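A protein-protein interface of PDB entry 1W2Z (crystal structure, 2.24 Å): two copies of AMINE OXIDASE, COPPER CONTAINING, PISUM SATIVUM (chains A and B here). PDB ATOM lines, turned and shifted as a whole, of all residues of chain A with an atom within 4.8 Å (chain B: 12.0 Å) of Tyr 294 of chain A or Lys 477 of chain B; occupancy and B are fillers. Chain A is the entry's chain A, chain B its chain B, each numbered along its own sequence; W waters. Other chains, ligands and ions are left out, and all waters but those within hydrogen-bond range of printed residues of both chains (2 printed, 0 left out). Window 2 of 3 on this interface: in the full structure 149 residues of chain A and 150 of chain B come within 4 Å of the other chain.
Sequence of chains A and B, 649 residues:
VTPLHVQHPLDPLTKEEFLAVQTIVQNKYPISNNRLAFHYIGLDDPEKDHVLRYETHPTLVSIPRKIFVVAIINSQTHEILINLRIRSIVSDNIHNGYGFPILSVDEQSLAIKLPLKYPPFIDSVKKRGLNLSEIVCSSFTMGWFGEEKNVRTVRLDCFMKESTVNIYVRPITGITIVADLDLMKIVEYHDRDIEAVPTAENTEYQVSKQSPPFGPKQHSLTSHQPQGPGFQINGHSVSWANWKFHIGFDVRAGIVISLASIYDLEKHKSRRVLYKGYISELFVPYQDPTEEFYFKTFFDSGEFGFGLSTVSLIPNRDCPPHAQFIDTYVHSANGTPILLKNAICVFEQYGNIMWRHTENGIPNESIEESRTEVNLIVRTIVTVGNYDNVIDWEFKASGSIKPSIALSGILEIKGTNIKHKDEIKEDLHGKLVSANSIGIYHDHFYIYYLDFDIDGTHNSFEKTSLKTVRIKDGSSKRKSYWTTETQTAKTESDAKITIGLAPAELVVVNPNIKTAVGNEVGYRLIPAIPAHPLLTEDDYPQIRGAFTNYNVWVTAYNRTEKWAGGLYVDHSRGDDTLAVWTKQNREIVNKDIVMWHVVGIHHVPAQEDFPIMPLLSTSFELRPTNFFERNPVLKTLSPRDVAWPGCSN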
ATOM      1  N   MET A 142      16.476 -25.510  -9.483  1.00  0.00           N
ATOM      2  CA  MET A 142      16.853 -25.948  -8.141  1.00  0.00           C
ATOM      3  C   MET A 142      17.351 -27.394  -8.099  1.00  0.00           C
ATOM      4  O   MET A 142      17.704 -27.884  -7.027  1.00  0.00           O
ATOM      5  CB  MET A 142      15.592 -25.978  -7.256  1.00  0.00           C
ATOM      6  CG  MET A 142      15.076 -24.697  -6.785  1.00  0.00           C
ATOM      7  SD  MET A 142      13.546 -24.974  -5.838  1.00  0.00           S
ATOM      8  CE  MET A 142      14.195 -25.575  -4.246  1.00  0.00           C
ATOM      9  N   PHE A 145      18.357 -32.815  -4.570  1.00  0.00           N
ATOM     10  CA  PHE A 145      19.387 -33.018  -3.554  1.00  0.00           C
ATOM     11  C   PHE A 145      19.005 -34.140  -2.590  1.00  0.00           C
ATOM     12  O   PHE A 145      19.244 -34.039  -1.390  1.00  0.00           O
ATOM     13  CB  PHE A 145      19.685 -31.703  -2.799  1.00  0.00           C
ATOM     14  CG  PHE A 145      20.362 -30.686  -3.652  1.00  0.00           C
ATOM     15  CD1 PHE A 145      21.729 -30.632  -3.709  1.00  0.00           C
ATOM     16  CD2 PHE A 145      19.622 -29.840  -4.471  1.00  0.00           C
ATOM     17  CE1 PHE A 145      22.354 -29.759  -4.531  1.00  0.00           C
ATOM     18  CE2 PHE A 145      20.233 -28.957  -5.292  1.00  0.00           C
ATOM     19  CZ  PHE A 145      21.618 -28.913  -5.336  1.00  0.00           C
ATOM     20  N   ARG A 155      13.852 -21.407  -7.551  1.00  0.00           N
ATOM     21  CA  ARG A 155      14.249 -20.320  -6.674  1.00  0.00           C
ATOM     22  C   ARG A 155      14.112 -19.007  -7.441  1.00  0.00           C
ATOM     23  O   ARG A 155      14.439 -18.937  -8.611  1.00  0.00           O
ATOM     24  CB  ARG A 155      15.700 -20.515  -6.204  1.00  0.00           C
ATOM     25  CG  ARG A 155      15.873 -21.584  -5.110  1.00  0.00           C
ATOM     26  CD  ARG A 155      15.516 -21.095  -3.697  1.00  0.00           C
ATOM     27  NE  ARG A 155      16.424 -20.053  -3.178  1.00  0.00           N
ATOM     28  CZ  ARG A 155      17.402 -20.251  -2.292  1.00  0.00           C
ATOM     29  NH1 ARG A 155      17.650 -21.456  -1.806  1.00  0.00           N
ATOM     30  NH2 ARG A 155      18.153 -19.233  -1.904  1.00  0.00           N
ATOM     31  N   ASP A 288      29.307 -22.318  -4.565  1.00  0.00           N
ATOM     32  CA  ASP A 288      28.908 -21.706  -3.316  1.00  0.00           C
ATOM     33  C   ASP A 288      27.857 -22.610  -2.646  1.00  0.00           C
ATOM     34  O   ASP A 288      26.707 -22.664  -3.083  1.00  0.00           O
ATOM     35  CB  ASP A 288      28.341 -20.318  -3.604  1.00  0.00           C
ATOM     36  CG  ASP A 288      27.746 -19.656  -2.384  1.00  0.00           C
ATOM     37  OD1 ASP A 288      27.616 -20.323  -1.345  1.00  0.00           O
ATOM     38  OD2 ASP A 288      27.342 -18.473  -2.392  1.00  0.00           O
ATOM     39  N   PRO A 289      28.251 -23.301  -1.577  1.00  0.00           N
ATOM     40  CA  PRO A 289      27.403 -24.313  -0.946  1.00  0.00           C
ATOM     41  C   PRO A 289      26.401 -23.777   0.045  1.00  0.00           C
ATOM     42  O   PRO A 289      25.679 -24.598   0.596  1.00  0.00           O
ATOM     43  CB  PRO A 289      28.426 -25.172  -0.186  1.00  0.00           C
ATOM     44  CG  PRO A 289      29.423 -24.199   0.236  1.00  0.00           C
ATOM     45  CD  PRO A 289      29.541 -23.195  -0.882  1.00  0.00           C
ATOM     46  N   THR A 290      26.394 -22.479   0.318  1.00  0.00           N
ATOM     47  CA  THR A 290      25.422 -21.890   1.252  1.00  0.00           C
ATOM     48  C   THR A 290      24.044 -21.890   0.620  1.00  0.00           C
ATOM     49  O   THR A 290      23.913 -22.172  -0.582  1.00  0.00           O
ATOM     50  CB  THR A 290      25.810 -20.442   1.575  1.00  0.00           C
ATOM     51  OG1 THR A 290      25.816 -19.660   0.358  1.00  0.00           O
ATOM     52  CG2 THR A 290      27.256 -20.385   2.084  1.00  0.00           C
ATOM     53  N   GLU A 291      23.053 -21.528   1.428  1.00  0.00           N
ATOM     54  CA  GLU A 291      21.667 -21.485   1.040  1.00  0.00           C
ATOM     55  C   GLU A 291      21.419 -20.562  -0.155  1.00  0.00           C
ATOM     56  O   GLU A 291      20.490 -20.785  -0.931  1.00  0.00           O
ATOM     57  CB  GLU A 291      20.825 -21.061   2.256  1.00  0.00           C
ATOM     58  CG  GLU A 291      19.327 -21.037   1.992  1.00  0.00           C
ATOM     59  CD  GLU A 291      18.477 -21.176   3.245  1.00  0.00           C
ATOM     60  OE1 GLU A 291      19.025 -21.455   4.333  1.00  0.00           O
ATOM     61  OE2 GLU A 291      17.246 -21.014   3.134  1.00  0.00           O
ATOM     62  N   GLU A 292      22.274 -19.553  -0.328  1.00  0.00           N
ATOM     63  CA  GLU A 292      22.141 -18.589  -1.421  1.00  0.00           C
ATOM     64  C   GLU A 292      22.313 -19.193  -2.811  1.00  0.00           C
ATOM     65  O   GLU A 292      21.638 -18.792  -3.746  1.00  0.00           O
ATOM     66  CB  GLU A 292      23.159 -17.447  -1.215  1.00  0.00           C
ATOM     67  CG  GLU A 292      22.922 -16.192  -2.060  1.00  0.00           C
ATOM     68  CD  GLU A 292      21.611 -15.488  -1.761  1.00  0.00           C
ATOM     69  OE1 GLU A 292      21.095 -15.650  -0.646  1.00  0.00           O
ATOM     70  OE2 GLU A 292      21.094 -14.760  -2.645  1.00  0.00           O
ATOM     71  N   PHE A 293      23.212 -20.150  -2.963  1.00  0.00           N
ATOM     72  CA  PHE A 293      23.569 -20.643  -4.298  1.00  0.00           C
ATOM     73  C   PHE A 293      23.791 -22.160  -4.463  1.00  0.00           C
ATOM     74  O   PHE A 293      24.153 -22.604  -5.550  1.00  0.00           O
ATOM     75  CB  PHE A 293      24.825 -19.886  -4.755  1.00  0.00           C
ATOM     76  CG  PHE A 293      24.528 -18.567  -5.382  1.00  0.00           C
ATOM     77  CD1 PHE A 293      23.828 -18.503  -6.579  1.00  0.00           C
ATOM     78  CD2 PHE A 293      24.907 -17.390  -4.769  1.00  0.00           C
ATOM     79  CE1 PHE A 293      23.530 -17.271  -7.161  1.00  0.00           C
ATOM     80  CE2 PHE A 293      24.614 -16.152  -5.347  1.00  0.00           C
ATOM     81  CZ  PHE A 293      23.932 -16.093  -6.529  1.00  0.00           C
ATOM     82  N   TYR A 294      23.555 -22.962  -3.420  1.00  0.00           N
ATOM     83  CA  TYR A 294      23.900 -24.402  -3.455  1.00  0.00           C
ATOM     84  C   TYR A 294      23.223 -25.136  -4.641  1.00  0.00           C
ATOM     85  O   TYR A 294      23.761 -26.070  -5.208  1.00  0.00           O
ATOM     86  CB  TYR A 294      23.522 -25.100  -2.128  1.00  0.00           C
ATOM     87  CG  TYR A 294      22.031 -25.346  -2.012  1.00  0.00           C
ATOM     88  CD1 TYR A 294      21.181 -24.383  -1.450  1.00  0.00           C
ATOM     89  CD2 TYR A 294      21.459 -26.533  -2.488  1.00  0.00           C
ATOM     90  CE1 TYR A 294      19.782 -24.596  -1.370  1.00  0.00           C
ATOM     91  CE2 TYR A 294      20.063 -26.760  -2.415  1.00  0.00           C
ATOM     92  CZ  TYR A 294      19.233 -25.778  -1.871  1.00  0.00           C
ATOM     93  OH  TYR A 294      17.879 -26.015  -1.789  1.00  0.00           O
ATOM     94  N   PHE A 295      22.023 -24.686  -4.955  1.00  0.00           N
ATOM     95  CA  PHE A 295      21.117 -25.272  -5.946  1.00  0.00           C
ATOM     96  C   PHE A 295      21.392 -24.843  -7.401  1.00  0.00           C
ATOM     97  O   PHE A 295      20.772 -25.372  -8.323  1.00  0.00           O
ATOM     98  CB  PHE A 295      19.711 -24.792  -5.602  1.00  0.00           C
ATOM     99  CG  PHE A 295      19.594 -23.298  -5.619  1.00  0.00           C
ATOM    100  CD1 PHE A 295      19.264 -22.633  -6.783  1.00  0.00           C
ATOM    101  CD2 PHE A 295      19.884 -22.555  -4.488  1.00  0.00           C
ATOM    102  CE1 PHE A 295      19.204 -21.250  -6.805  1.00  0.00           C
ATOM    103  CE2 PHE A 295      19.837 -21.181  -4.511  1.00  0.00           C
ATOM    104  CZ  PHE A 295      19.497 -20.527  -5.658  1.00  0.00           C
ATOM    105  N   LYS A 296      22.277 -23.866  -7.597  1.00  0.00           N
ATOM    106  CA  LYS A 296      22.489 -23.293  -8.924  1.00  0.00           C
ATOM    107  C   LYS A 296      23.565 -24.038  -9.731  1.00  0.00           C
ATOM    108  O   LYS A 296      24.772 -23.776  -9.610  1.00  0.00           O
ATOM    109  CB  LYS A 296      22.791 -21.788  -8.878  1.00  0.00           C
ATOM    110  CG  LYS A 296      22.021 -21.009  -9.966  1.00  0.00           C
ATOM    111  CD  LYS A 296      22.793 -19.830 -10.574  1.00  0.00           C
ATOM    112  CE  LYS A 296      22.697 -19.783 -12.119  1.00  0.00           C
ATOM    113  NZ  LYS A 296      21.856 -18.676 -12.644  1.00  0.00           N
ATOM    114  N   THR A 297      23.093 -24.986 -10.531  1.00  0.00           N
ATOM    115  CA  THR A 297      23.921 -25.740 -11.459  1.00  0.00           C
ATOM    116  C   THR A 297      23.087 -25.989 -12.719  1.00  0.00           C
ATOM    117  O   THR A 297      22.623 -27.106 -12.946  1.00  0.00           O
ATOM    118  CB  THR A 297      24.371 -27.096 -10.854  1.00  0.00           C
ATOM    119  OG1 THR A 297      23.244 -27.979 -10.718  1.00  0.00           O
ATOM    120  CG2 THR A 297      24.921 -26.958  -9.452  1.00  0.00           C
ATOM    121  N   TYR A 540      25.072 -34.459  -5.820  1.00  0.00           N
ATOM    122  CA  TYR A 540      23.815 -34.550  -6.550  1.00  0.00           C
ATOM    123  C   TYR A 540      23.878 -33.898  -7.922  1.00  0.00           C
ATOM    124  O   TYR A 540      23.449 -34.497  -8.910  1.00  0.00           O
ATOM    125  CB  TYR A 540      22.663 -33.976  -5.708  1.00  0.00           C
ATOM    126  CG  TYR A 540      22.537 -34.648  -4.371  1.00  0.00           C
ATOM    127  CD1 TYR A 540      21.935 -35.896  -4.250  1.00  0.00           C
ATOM    128  CD2 TYR A 540      23.012 -34.041  -3.230  1.00  0.00           C
ATOM    129  CE1 TYR A 540      21.816 -36.513  -3.018  1.00  0.00           C
ATOM    130  CE2 TYR A 540      22.905 -34.651  -1.997  1.00  0.00           C
ATOM    131  CZ  TYR A 540      22.304 -35.889  -1.882  1.00  0.00           C
ATOM    132  OH  TYR A 540      22.220 -36.491  -0.612  1.00  0.00           O
ATOM    133  N   VAL B 469      36.520 -29.455  -2.047  1.00  0.00           N
ATOM    134  CA  VAL B 469      36.178 -29.587  -0.636  1.00  0.00           C
ATOM    135  C   VAL B 469      34.921 -30.448  -0.498  1.00  0.00           C
ATOM    136  O   VAL B 469      33.915 -30.182  -1.127  1.00  0.00           O
ATOM    137  CB  VAL B 469      35.899 -28.205   0.023  1.00  0.00           C
ATOM    138  CG1 VAL B 469      35.545 -28.370   1.522  1.00  0.00           C
ATOM    139  CG2 VAL B 469      37.092 -27.242  -0.146  1.00  0.00           C
ATOM    140  N   ARG B 470      34.982 -31.465   0.348  1.00  0.00           N
ATOM    141  CA  ARG B 470      33.836 -32.309   0.638  1.00  0.00           C
ATOM    142  C   ARG B 470      33.115 -31.803   1.888  1.00  0.00           C
ATOM    143  O   ARG B 470      33.744 -31.558   2.914  1.00  0.00           O
ATOM    144  CB  ARG B 470      34.311 -33.751   0.862  1.00  0.00           C
ATOM    145  CG  ARG B 470      33.158 -34.751   1.042  1.00  0.00           C
ATOM    146  CD  ARG B 470      33.597 -36.192   1.206  1.00  0.00           C
ATOM    147  NE  ARG B 470      33.831 -36.850  -0.077  1.00  0.00           N
ATOM    148  CZ  ARG B 470      32.879 -37.296  -0.891  1.00  0.00           C
ATOM    149  NH1 ARG B 470      31.589 -37.154  -0.574  1.00  0.00           N
ATOM    150  NH2 ARG B 470      33.222 -37.880  -2.036  1.00  0.00           N
ATOM    151  N   ILE B 471      31.799 -31.623   1.805  1.00  0.00           N
ATOM    152  CA  ILE B 471      30.999 -31.282   2.979  1.00  0.00           C
ATOM    153  C   ILE B 471      30.351 -32.586   3.513  1.00  0.00           C
ATOM    154  O   ILE B 471      29.584 -33.254   2.795  1.00  0.00           O
ATOM    155  CB  ILE B 471      29.892 -30.243   2.615  1.00  0.00           C
ATOM    156  CG1 ILE B 471      30.494 -28.951   2.044  1.00  0.00           C
ATOM    157  CG2 ILE B 471      29.009 -29.917   3.830  1.00  0.00           C
ATOM    158  CD1 ILE B 471      29.573 -28.228   1.113  1.00  0.00           C
ATOM    159  N   LYS B 472      30.644 -32.934   4.761  1.00  0.00           N
ATOM    160  CA  LYS B 472      30.119 -34.157   5.387  1.00  0.00           C
ATOM    161  C   LYS B 472      29.161 -33.860   6.536  1.00  0.00           C
ATOM    162  O   LYS B 472      28.276 -34.656   6.836  1.00  0.00           O
ATOM    163  CB  LYS B 472      31.284 -34.996   5.941  1.00  0.00           C
ATOM    164  CG  LYS B 472      31.548 -36.304   5.208  1.00  0.00           C
ATOM    165  CD  LYS B 472      33.038 -36.726   5.362  1.00  0.00           C
ATOM    166  CE  LYS B 472      33.258 -38.245   5.225  1.00  0.00           C
ATOM    167  NZ  LYS B 472      34.093 -38.584   4.036  1.00  0.00           N
ATOM    168  N   ASP B 473      29.357 -32.711   7.178  1.00  0.00           N
ATOM    169  CA  ASP B 473      28.768 -32.417   8.487  1.00  0.00           C
ATOM    170  C   ASP B 473      27.327 -31.886   8.499  1.00  0.00           C
ATOM    171  O   ASP B 473      26.882 -31.405   9.527  1.00  0.00           O
ATOM    172  CB  ASP B 473      29.679 -31.440   9.247  1.00  0.00           C
ATOM    173  CG  ASP B 473      29.781 -30.068   8.585  1.00  0.00           C
ATOM    174  OD1 ASP B 473      29.208 -29.847   7.497  1.00  0.00           O
ATOM    175  OD2 ASP B 473      30.437 -29.136   9.090  1.00  0.00           O
ATOM    176  N   GLY B 474      26.611 -31.955   7.373  1.00  0.00           N
ATOM    177  CA  GLY B 474      25.212 -31.543   7.314  1.00  0.00           C
ATOM    178  C   GLY B 474      24.941 -30.048   7.143  1.00  0.00           C
ATOM    179  O   GLY B 474      23.772 -29.619   7.144  1.00  0.00           O
ATOM    180  N   SER B 475      25.996 -29.255   6.944  1.00  0.00           N
ATOM    181  CA  SER B 475      25.872 -27.789   6.851  1.00  0.00           C
ATOM    182  C   SER B 475      25.360 -27.292   5.467  1.00  0.00           C
ATOM    183  O   SER B 475      25.023 -26.118   5.303  1.00  0.00           O
ATOM    184  CB  SER B 475      27.211 -27.122   7.204  1.00  0.00           C
ATOM    185  OG  SER B 475      28.182 -27.323   6.184  1.00  0.00           O
ATOM    186  N   SER B 476      25.317 -28.187   4.485  1.00  0.00           N
ATOM    187  CA  SER B 476      24.806 -27.875   3.158  1.00  0.00           C
ATOM    188  C   SER B 476      24.126 -29.087   2.565  1.00  0.00           C
ATOM    189  O   SER B 476      24.431 -30.223   2.929  1.00  0.00           O
ATOM    190  CB  SER B 476      25.968 -27.478   2.243  1.00  0.00           C
ATOM    191  OG  SER B 476      25.508 -27.031   0.981  1.00  0.00           O
ATOM    192  N   LYS B 477      23.218 -28.838   1.637  1.00  0.00           N
ATOM    193  CA  LYS B 477      22.630 -29.908   0.835  1.00  0.00           C
ATOM    194  C   LYS B 477      23.607 -30.412  -0.226  1.00  0.00           C
ATOM    195  O   LYS B 477      23.463 -31.525  -0.751  1.00  0.00           O
ATOM    196  CB  LYS B 477      21.329 -29.409   0.214  1.00  0.00           C
ATOM    197  CG  LYS B 477      20.230 -29.268   1.271  1.00  0.00           C
ATOM    198  CD  LYS B 477      18.897 -28.813   0.663  1.00  0.00           C
ATOM    199  CE  LYS B 477      17.870 -28.460   1.751  1.00  0.00           C
ATOM    200  NZ  LYS B 477      17.731 -29.575   2.734  1.00  0.00           N
ATOM    201  N   ARG B 478      24.588 -29.585  -0.562  1.00  0.00           N
ATOM    202  CA  ARG B 478      25.643 -29.997  -1.474  1.00  0.00           C
ATOM    203  C   ARG B 478      26.640 -30.879  -0.728  1.00  0.00           C
ATOM    204  O   ARG B 478      26.925 -30.646   0.424  1.00  0.00           O
ATOM    205  CB  ARG B 478      26.353 -28.778  -2.065  1.00  0.00           C
ATOM    206  CG  ARG B 478      25.631 -28.191  -3.267  1.00  0.00           C
ATOM    207  CD  ARG B 478      25.944 -28.893  -4.581  1.00  0.00           C
ATOM    208  NE  ARG B 478      27.290 -28.559  -5.058  1.00  0.00           N
ATOM    209  CZ  ARG B 478      27.631 -27.376  -5.596  1.00  0.00           C
ATOM    210  NH1 ARG B 478      26.743 -26.413  -5.749  1.00  0.00           N
ATOM    211  NH2 ARG B 478      28.878 -27.160  -5.987  1.00  0.00           N
ATOM    212  N   LYS B 479      27.154 -31.888  -1.405  1.00  0.00           N
ATOM    213  CA  LYS B 479      28.232 -32.712  -0.898  1.00  0.00           C
ATOM    214  C   LYS B 479      29.594 -32.144  -1.220  1.00  0.00           C
ATOM    215  O   LYS B 479      30.574 -32.566  -0.623  1.00  0.00           O
ATOM    216  CB  LYS B 479      28.148 -34.125  -1.492  1.00  0.00           C
ATOM    217  CG  LYS B 479      26.977 -34.932  -0.938  1.00  0.00           C
ATOM    218  CD  LYS B 479      27.168 -36.438  -1.130  1.00  0.00           C
ATOM    219  CE  LYS B 479      26.043 -37.228  -0.457  1.00  0.00           C
ATOM    220  NZ  LYS B 479      24.918 -37.368  -1.407  1.00  0.00           N
ATOM    221  N   SER B 480      29.683 -31.214  -2.174  1.00  0.00           N
ATOM    222  CA  SER B 480      30.993 -30.745  -2.617  1.00  0.00           C
ATOM    223  C   SER B 480      30.987 -29.416  -3.345  1.00  0.00           C
ATOM    224  O   SER B 480      29.980 -28.966  -3.886  1.00  0.00           O
ATOM    225  CB  SER B 480      31.670 -31.805  -3.500  1.00  0.00           C
ATOM    226  OG  SER B 480      31.132 -31.814  -4.806  1.00  0.00           O
ATOM    227  N   TYR B 481      32.148 -28.799  -3.356  1.00  0.00           N
ATOM    228  CA  TYR B 481      32.379 -27.614  -4.150  1.00  0.00           C
ATOM    229  C   TYR B 481      33.869 -27.479  -4.312  1.00  0.00           C
ATOM    230  O   TYR B 481      34.623 -28.157  -3.620  1.00  0.00           O
ATOM    231  CB  TYR B 481      31.811 -26.382  -3.465  1.00  0.00           C
ATOM    232  CG  TYR B 481      32.468 -26.020  -2.157  1.00  0.00           C
ATOM    233  CD1 TYR B 481      32.119 -26.676  -0.965  1.00  0.00           C
ATOM    234  CD2 TYR B 481      33.417 -25.008  -2.092  1.00  0.00           C
ATOM    235  CE1 TYR B 481      32.706 -26.318   0.257  1.00  0.00           C
ATOM    236  CE2 TYR B 481      34.025 -24.654  -0.886  1.00  0.00           C
ATOM    237  CZ  TYR B 481      33.661 -25.317   0.283  1.00  0.00           C
ATOM    238  OH  TYR B 481      34.266 -24.969   1.458  1.00  0.00           O
ATOM    239  N   TRP B 482      34.292 -26.619  -5.229  1.00  0.00           N
ATOM    240  CA  TRP B 482      35.703 -26.259  -5.317  1.00  0.00           C
ATOM    241  C   TRP B 482      35.943 -24.808  -4.948  1.00  0.00           C
ATOM    242  O   TRP B 482      35.043 -23.975  -5.023  1.00  0.00           O
ATOM    243  CB  TRP B 482      36.305 -26.625  -6.674  1.00  0.00           C
ATOM    244  CG  TRP B 482      35.802 -25.912  -7.922  1.00  0.00           C
ATOM    245  CD1 TRP B 482      34.939 -26.417  -8.852  1.00  0.00           C
ATOM    246  CD2 TRP B 482      36.228 -24.635  -8.429  1.00  0.00           C
ATOM    247  NE1 TRP B 482      34.768 -25.525  -9.884  1.00  0.00           N
ATOM    248  CE2 TRP B 482      35.546 -24.422  -9.658  1.00  0.00           C
ATOM    249  CE3 TRP B 482      37.101 -23.633  -7.961  1.00  0.00           C
ATOM    250  CZ2 TRP B 482      35.721 -23.261 -10.436  1.00  0.00           C
ATOM    251  CZ3 TRP B 482      37.270 -22.477  -8.727  1.00  0.00           C
ATOM    252  CH2 TRP B 482      36.571 -22.304  -9.959  1.00  0.00           C
HETATM  253  O   HOH W   1      26.719 -23.203  -5.739  1.00  0.00           O
HETATM  254  O   HOH W   2      21.359 -33.225   0.300  1.00  0.00           O
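Of the 14 printed residues of chain B, 6 touch a printed residue of chain A. Hydrophobic or aromatic side chains of chain B that line the printed part of chain A: Ile 471 and Tyr 481. Of the 14 printed residues of chain A, 4 touch a printed residue of chain B. Along chain A the printed residues that touch a printed residue of chain B span positions 145 to 540. Among the printed residues, 9 pairs touch across the chains. Among the printed residues, no Asp or Glu carboxylate lies within 4 Å of a Lys or Arg side-chain nitrogen of the other chain.
The backbone carbonyl oxygen (O) of Pro 289 of chain A is in hydrogen-bond range of the side-chain hydroxyl (OG) of Ser 476 of chain B, at 2.5 Å. O of Tyr 294 of chain A lies within hydrogen-bond range of NH1 of Arg 478 of chain B (3.1 Å). NZ of Lys 479 of chain B lies within hydrogen-bond range of OH of Tyr 540 of chain A (2.9 Å).
O of Lys 477 of chain B touches CD1 of Phe 145 of chain A, 3.5 Å away. Arg 478 of chain B touches Phe 145 of chain A. Ile 471 of chain B touches Pro 289 of chain A. CG of Pro 289 of chain A touches CD1 of Tyr 481 of chain B (3.9 Å). OH of Tyr 294 of chain A touches CD of Lys 477 of chain B (3.9 Å). Tyr 540 of chain A touches Lys 477 of chain B (CE2 to O, 3.4 Å).
Water W1 lies within hydrogen-bond range of the backbone carbonyl oxygen (O) of Phe 293 of chain A, the backbone carbonyl oxygen (O) of Asp 288 of chain A and the guanidinium group (NH1) of Arg 478 of chain B. Water W2 lies within hydrogen-bond range of O of Phe 145 of chain A (2.8 Å), O of Lys 477 of chain B (2.9 Å) and OH of Tyr 540 of chain A (3.5 Å).
No residue of chain B comes within 4 Å of Asp 288 of chain A. Of chain B, only Ile 471 (3.5 Å), Ser 476 (2.5 Å) and Tyr 481 (3.9 Å) come within 4 Å of Pro 289 of chain A. No residue of chain B comes within 4 Å of Thr 290 of chain A. No residue of chain B comes within 4 Å of Phe 293 of chain A. Of chain B, only Lys 477 (3.9 Å) and Arg 478 (3.1 Å) come within 4 Å of Tyr 294 of chain A. Thr 297 of chain A touches none of the printed residues of chain B. Arg 470 of chain B touches none of the printed residues of chain A. Of the printed residues of chain A, Ser 476 of chain B touches Pro 289 (2.5 Å). Lys 477 of chain B touches just these residues of chain A: Phe 145 (3.5 Å), Tyr 294 (3.9 Å) and Tyr 540 (3.4 Å). Of the printed residues of chain A, Tyr 481 of chain B touches Pro 289 (3.9 Å). The nearest printed residue of chain A that does not touch Ile 471 of chain B is Thr 290 of chain A (6.6 Å).
The backbone NH of Tyr 294 of chain A is in hydrogen-bond range of the backbone carbonyl oxygen of Asp 288 of chain A, at 3.2 Å. O of Tyr 481 of chain B lies within hydrogen-bond range of N of Val 469 of chain B (2.8 Å). N of Ile 471 of chain B lies within hydrogen-bond range of O of Lys 479 of chain B. The side-chain hydroxyl (OG) of Ser 476 of chain B lies within hydrogen-bond range of the backbone NH (N) of Arg 478 of chain B (3.1 Å). NE of Arg 478 of chain B is in hydrogen-bond range of O of Ser 480 of chain B.
No position is printed for both chains.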
